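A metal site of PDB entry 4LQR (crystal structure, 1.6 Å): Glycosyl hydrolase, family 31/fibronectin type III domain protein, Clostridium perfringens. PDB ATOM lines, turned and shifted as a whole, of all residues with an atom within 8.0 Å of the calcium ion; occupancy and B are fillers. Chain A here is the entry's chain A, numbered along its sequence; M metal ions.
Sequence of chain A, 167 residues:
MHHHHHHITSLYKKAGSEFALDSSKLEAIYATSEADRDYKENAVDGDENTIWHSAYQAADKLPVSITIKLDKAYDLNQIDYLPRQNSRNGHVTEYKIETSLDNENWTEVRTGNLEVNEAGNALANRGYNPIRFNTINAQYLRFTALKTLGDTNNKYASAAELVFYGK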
ATOM      1  N   SER A  23     -27.426  -0.008 -10.725  1.00  0.00           N
ATOM      2  CA  SER A  23     -26.393  -0.360 -11.720  1.00  0.00           C
ATOM      3  C   SER A  23     -26.938  -0.616 -13.123  1.00  0.00           C
ATOM      4  O   SER A  23     -26.172  -0.499 -14.085  1.00  0.00           O
ATOM      5  CB  SER A  23     -25.528  -1.543 -11.262  1.00  0.00           C
ATOM      6  OG  SER A  23     -24.794  -1.199 -10.107  1.00  0.00           O
ATOM      7  N   TYR A  39     -15.531  -9.161 -17.997  1.00  0.00           N
ATOM      8  CA  TYR A  39     -16.022  -8.188 -19.037  1.00  0.00           C
ATOM      9  C   TYR A  39     -16.143  -6.787 -18.477  1.00  0.00           C
ATOM     10  O   TYR A  39     -16.357  -6.576 -17.247  1.00  0.00           O
ATOM     11  CB  TYR A  39     -17.417  -8.633 -19.443  1.00  0.00           C
ATOM     12  CG  TYR A  39     -17.490 -10.039 -19.984  1.00  0.00           C
ATOM     13  CD1 TYR A  39     -16.603 -10.463 -20.981  1.00  0.00           C
ATOM     14  CD2 TYR A  39     -18.429 -10.923 -19.461  1.00  0.00           C
ATOM     15  CE1 TYR A  39     -16.665 -11.759 -21.495  1.00  0.00           C
ATOM     16  CE2 TYR A  39     -18.501 -12.221 -19.966  1.00  0.00           C
ATOM     17  CZ  TYR A  39     -17.634 -12.586 -20.978  1.00  0.00           C
ATOM     18  OH  TYR A  39     -17.724 -13.943 -21.413  1.00  0.00           O
ATOM     19  N   LYS A  40     -15.996  -5.808 -19.372  1.00  0.00           N
ATOM     20  CA  LYS A  40     -16.243  -4.411 -18.924  1.00  0.00           C
ATOM     21  C   LYS A  40     -17.611  -4.254 -18.226  1.00  0.00           C
ATOM     22  O   LYS A  40     -17.695  -3.512 -17.247  1.00  0.00           O
ATOM     23  CB  LYS A  40     -15.987  -3.438 -20.101  1.00  0.00           C
ATOM     24  CG  LYS A  40     -16.946  -3.630 -21.232  1.00  0.00           C
ATOM     25  CD  LYS A  40     -16.620  -2.721 -22.405  1.00  0.00           C
ATOM     26  CE  LYS A  40     -17.591  -2.804 -23.581  1.00  0.00           C
ATOM     27  NZ  LYS A  40     -17.334  -4.082 -24.351  1.00  0.00           N
ATOM     28  N   GLU A  41     -18.627  -4.945 -18.710  1.00  0.00           N
ATOM     29  CA  GLU A  41     -19.979  -4.791 -18.138  1.00  0.00           C
ATOM     30  C   GLU A  41     -19.954  -5.199 -16.660  1.00  0.00           C
ATOM     31  O   GLU A  41     -20.769  -4.726 -15.883  1.00  0.00           O
ATOM     32  CB  GLU A  41     -20.984  -5.640 -18.865  1.00  0.00           C
ATOM     33  CG  GLU A  41     -21.278  -5.248 -20.357  1.00  0.00           C
ATOM     34  CD  GLU A  41     -20.242  -5.687 -21.365  1.00  0.00           C
ATOM     35  OE1 GLU A  41     -19.262  -6.405 -21.011  1.00  0.00           O
ATOM     36  OE2 GLU A  41     -20.325  -5.214 -22.560  1.00  0.00           O
ATOM     37  N   ASN A  42     -19.020  -6.060 -16.262  1.00  0.00           N
ATOM     38  CA  ASN A  42     -19.003  -6.545 -14.895  1.00  0.00           C
ATOM     39  C   ASN A  42     -18.514  -5.456 -13.943  1.00  0.00           C
ATOM     40  O   ASN A  42     -18.668  -5.636 -12.682  1.00  0.00           O
ATOM     41  CB  ASN A  42     -18.053  -7.707 -14.716  1.00  0.00           C
ATOM     42  CG  ASN A  42     -18.546  -8.983 -15.394  1.00  0.00           C
ATOM     43  OD1 ASN A  42     -19.596  -9.017 -16.000  1.00  0.00           O
ATOM     44  ND2 ASN A  42     -17.716 -10.048 -15.341  1.00  0.00           N
ATOM     45  N   ALA A  43     -17.942  -4.312 -14.438  1.00  0.00           N
ATOM     46  CA  ALA A  43     -17.555  -3.271 -13.507  1.00  0.00           C
ATOM     47  C   ALA A  43     -18.747  -2.521 -13.000  1.00  0.00           C
ATOM     48  O   ALA A  43     -18.617  -1.769 -12.059  1.00  0.00           O
ATOM     49  CB  ALA A  43     -16.597  -2.254 -14.172  1.00  0.00           C
ATOM     50  N   VAL A  44     -19.884  -2.624 -13.661  1.00  0.00           N
ATOM     51  CA  VAL A  44     -21.080  -1.803 -13.321  1.00  0.00           C
ATOM     52  C   VAL A  44     -22.360  -2.636 -13.407  1.00  0.00           C
ATOM     53  O   VAL A  44     -23.412  -2.132 -13.790  1.00  0.00           O
ATOM     54  CB  VAL A  44     -21.186  -0.543 -14.228  1.00  0.00           C
ATOM     55  CG1 VAL A  44     -20.063   0.430 -13.915  1.00  0.00           C
ATOM     56  CG2 VAL A  44     -21.094  -0.912 -15.733  1.00  0.00           C
ATOM     57  N   ASP A  45     -22.261  -3.888 -12.931  1.00  0.00           N
ATOM     58  CA  ASP A  45     -23.449  -4.787 -12.955  1.00  0.00           C
ATOM     59  C   ASP A  45     -24.041  -4.939 -11.558  1.00  0.00           C
ATOM     60  O   ASP A  45     -25.021  -5.736 -11.446  1.00  0.00           O
ATOM     61  CB  ASP A  45     -23.128  -6.143 -13.547  1.00  0.00           C
ATOM     62  CG  ASP A  45     -22.059  -6.922 -12.721  1.00  0.00           C
ATOM     63  OD1 ASP A  45     -21.492  -6.405 -11.710  1.00  0.00           O
ATOM     64  OD2 ASP A  45     -21.782  -8.062 -13.141  1.00  0.00           O
ATOM     65  N   GLY A  46     -23.626  -4.141 -10.598  1.00  0.00           N
ATOM     66  CA  GLY A  46     -24.195  -4.213  -9.247  1.00  0.00           C
ATOM     67  C   GLY A  46     -23.863  -5.477  -8.523  1.00  0.00           C
ATOM     68  O   GLY A  46     -24.428  -5.741  -7.458  1.00  0.00           O
ATOM     69  N   ASP A  47     -22.949  -6.292  -9.059  1.00  0.00           N
ATOM     70  CA  ASP A  47     -22.545  -7.590  -8.406  1.00  0.00           C
ATOM     71  C   ASP A  47     -21.097  -7.462  -7.952  1.00  0.00           C
ATOM     72  O   ASP A  47     -20.147  -7.376  -8.782  1.00  0.00           O
ATOM     73  CB  ASP A  47     -22.751  -8.736  -9.406  1.00  0.00           C
ATOM     74  CG  ASP A  47     -22.503 -10.148  -8.802  1.00  0.00           C
ATOM     75  OD1 ASP A  47     -21.774 -10.232  -7.778  1.00  0.00           O
ATOM     76  OD2 ASP A  47     -23.025 -11.085  -9.514  1.00  0.00           O
ATOM     77  N   GLU A  48     -20.931  -7.467  -6.646  1.00  0.00           N
ATOM     78  CA  GLU A  48     -19.592  -7.355  -6.059  1.00  0.00           C
ATOM     79  C   GLU A  48     -18.658  -8.535  -6.427  1.00  0.00           C
ATOM     80  O   GLU A  48     -17.422  -8.383  -6.292  1.00  0.00           O
ATOM     81  CB  GLU A  48     -19.618  -7.242  -4.495  1.00  0.00           C
ATOM     82  CG  GLU A  48     -20.404  -5.997  -4.071  1.00  0.00           C
ATOM     83  CD  GLU A  48     -20.350  -5.764  -2.585  1.00  0.00           C
ATOM     84  OE1 GLU A  48     -19.938  -6.662  -1.840  1.00  0.00           O
ATOM     85  OE2 GLU A  48     -20.722  -4.648  -2.149  1.00  0.00           O
ATOM     86  N   ASN A  49     -19.261  -9.640  -6.848  1.00  0.00           N
ATOM     87  CA  ASN A  49     -18.532 -10.843  -7.138  1.00  0.00           C
ATOM     88  C   ASN A  49     -17.992 -10.909  -8.543  1.00  0.00           C
ATOM     89  O   ASN A  49     -17.197 -11.820  -8.818  1.00  0.00           O
ATOM     90  CB  ASN A  49     -19.365 -12.105  -6.769  1.00  0.00           C
ATOM     91  CG  ASN A  49     -20.042 -11.950  -5.369  1.00  0.00           C
ATOM     92  OD1 ASN A  49     -19.398 -12.173  -4.312  1.00  0.00           O
ATOM     93  ND2 ASN A  49     -21.310 -11.440  -5.363  1.00  0.00           N
ATOM     94  N   THR A  50     -18.437 -10.045  -9.445  1.00  0.00           N
ATOM     95  CA  THR A  50     -17.950 -10.069 -10.842  1.00  0.00           C
ATOM     96  C   THR A  50     -17.074  -8.835 -11.030  1.00  0.00           C
ATOM     97  O   THR A  50     -17.348  -7.786 -10.385  1.00  0.00           O
ATOM     98  CB  THR A  50     -19.106  -9.928 -11.850  1.00  0.00           C
ATOM     99  OG1 THR A  50     -19.755  -8.664 -11.636  1.00  0.00           O
ATOM    100  CG2 THR A  50     -20.144 -11.099 -11.671  1.00  0.00           C
ATOM    101  N   ILE A  51     -16.033  -8.967 -11.859  1.00  0.00           N
ATOM    102  CA  ILE A  51     -15.068  -7.903 -12.089  1.00  0.00           C
ATOM    103  C   ILE A  51     -14.866  -7.687 -13.578  1.00  0.00           C
ATOM    104  O   ILE A  51     -15.012  -8.605 -14.404  1.00  0.00           O
ATOM    105  CB  ILE A  51     -13.686  -8.170 -11.443  1.00  0.00           C
ATOM    106  CG1 ILE A  51     -12.967  -9.334 -12.135  1.00  0.00           C
ATOM    107  CG2 ILE A  51     -13.909  -8.500  -9.927  1.00  0.00           C
ATOM    108  CD1 ILE A  51     -11.596  -9.548 -11.518  1.00  0.00           C
ATOM    109  N   TRP A  52     -14.519  -6.431 -13.877  1.00  0.00           N
ATOM    110  CA  TRP A  52     -13.748  -6.167 -15.146  1.00  0.00           C
ATOM    111  C   TRP A  52     -12.303  -6.353 -14.817  1.00  0.00           C
ATOM    112  O   TRP A  52     -11.804  -5.940 -13.742  1.00  0.00           O
ATOM    113  CB  TRP A  52     -13.988  -4.695 -15.568  1.00  0.00           C
ATOM    114  CG  TRP A  52     -13.006  -4.268 -16.667  1.00  0.00           C
ATOM    115  CD1 TRP A  52     -12.776  -4.887 -17.879  1.00  0.00           C
ATOM    116  CD2 TRP A  52     -12.145  -3.112 -16.625  1.00  0.00           C
ATOM    117  NE1 TRP A  52     -11.745  -4.179 -18.582  1.00  0.00           N
ATOM    118  CE2 TRP A  52     -11.343  -3.141 -17.777  1.00  0.00           C
ATOM    119  CE3 TRP A  52     -11.863  -2.163 -15.614  1.00  0.00           C
ATOM    120  CZ2 TRP A  52     -10.386  -2.165 -18.033  1.00  0.00           C
ATOM    121  CZ3 TRP A  52     -10.930  -1.146 -15.893  1.00  0.00           C
ATOM    122  CH2 TRP A  52     -10.215  -1.138 -17.099  1.00  0.00           C
ATOM    123  N   LEU A  82     -14.858  -0.174  -6.041  1.00  0.00           N
ATOM    124  CA  LEU A  82     -14.765  -1.384  -5.177  1.00  0.00           C
ATOM    125  C   LEU A  82     -13.656  -2.284  -5.781  1.00  0.00           C
ATOM    126  O   LEU A  82     -13.830  -2.744  -6.897  1.00  0.00           O
ATOM    127  CB  LEU A  82     -16.101  -2.156  -5.165  1.00  0.00           C
ATOM    128  CG  LEU A  82     -16.023  -3.368  -4.166  1.00  0.00           C
ATOM    129  CD1 LEU A  82     -15.925  -2.902  -2.699  1.00  0.00           C
ATOM    130  CD2 LEU A  82     -17.351  -4.201  -4.403  1.00  0.00           C
ATOM    131  N   ALA A 159     -11.758  -4.013 -11.575  1.00  0.00           N
ATOM    132  CA  ALA A 159     -12.714  -3.274 -10.719  1.00  0.00           C
ATOM    133  C   ALA A 159     -13.872  -4.234 -10.478  1.00  0.00           C
ATOM    134  O   ALA A 159     -14.441  -4.709 -11.478  1.00  0.00           O
ATOM    135  CB  ALA A 159     -13.237  -2.007 -11.418  1.00  0.00           C
ATOM    136  N   ALA A 160     -14.294  -4.372  -9.211  1.00  0.00           N
ATOM    137  CA  ALA A 160     -15.468  -5.207  -8.938  1.00  0.00           C
ATOM    138  C   ALA A 160     -16.751  -4.394  -9.179  1.00  0.00           C
ATOM    139  O   ALA A 160     -17.697  -4.915  -9.724  1.00  0.00           O
ATOM    140  CB  ALA A 160     -15.432  -5.761  -7.516  1.00  0.00           C
ATOM    141  N   GLU A 161     -16.758  -3.118  -8.771  1.00  0.00           N
ATOM    142  CA  GLU A 161     -17.883  -2.222  -9.013  1.00  0.00           C
ATOM    143  C   GLU A 161     -17.394  -0.805  -9.068  1.00  0.00           C
ATOM    144  O   GLU A 161     -16.466  -0.415  -8.344  1.00  0.00           O
ATOM    145  CB  GLU A 161     -18.889  -2.315  -7.814  1.00  0.00           C
ATOM    146  CG  GLU A 161     -19.811  -3.552  -7.961  1.00  0.00           C
ATOM    147  CD  GLU A 161     -20.640  -3.557  -9.267  1.00  0.00           C
ATOM    148  OE1 GLU A 161     -21.436  -2.596  -9.500  1.00  0.00           O
ATOM    149  OE2 GLU A 161     -20.560  -4.463 -10.097  1.00  0.00           O
ATOM    150  N   LEU A 162     -18.132  -0.009  -9.843  1.00  0.00           N
ATOM    151  CA  LEU A 162     -18.029   1.456  -9.838  1.00  0.00           C
ATOM    152  C   LEU A 162     -19.432   1.938  -9.502  1.00  0.00           C
ATOM    153  O   LEU A 162     -20.371   1.721 -10.281  1.00  0.00           O
ATOM    154  CB  LEU A 162     -17.551   2.024 -11.188  1.00  0.00           C
ATOM    155  CG  LEU A 162     -16.222   1.512 -11.693  1.00  0.00           C
ATOM    156  CD1 LEU A 162     -16.003   2.112 -13.063  1.00  0.00           C
ATOM    157  CD2 LEU A 162     -15.097   1.920 -10.742  1.00  0.00           C
HETATM  158 CA    CA M   1     -19.326  -6.380 -10.676  1.00  0.00          CA
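The side-chain amide nitrogen of Asn 42 sits close to the backbone carbonyl oxygen of Ile 51, 3.2 Å away. The side-chain carboxylate (OD1) of Asp 47 sits at hydrogen-bond distance from the side-chain amide nitrogen (ND2) of Asn 49 (2.7 Å). OE1 of Glu 161 lies within hydrogen-bond range of N of Gly 46, at 2.9 Å. The backbone carbonyl oxygen (O) of Glu 161 sits at hydrogen-bond distance from the backbone NH (N) of Leu 82, at 2.8 Å. The backbone carbonyl oxygen (O) of Leu 82 lies within hydrogen-bond range of the backbone NH (N) of Ala 160 (2.9 Å).
O of Asn 42 binds the calcium ion. The backbone carbonyl oxygen (O) of Asp 47 is bound to the calcium ion. OE2 of Glu 161 is bound to the calcium ion (2.4 Å). The backbone carbonyl oxygen (O) of Ala 160 binds the calcium ion. The side-chain carboxylate (OD1) of Asp 45 is bound to the calcium ion (2.4 Å). The calcium ion is bound by O of Thr 50, 2.4 Å away. The calcium ion is bound by OG1 of Thr 50 (2.5 Å). The calcium ion has seven donor atoms within binding distance.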
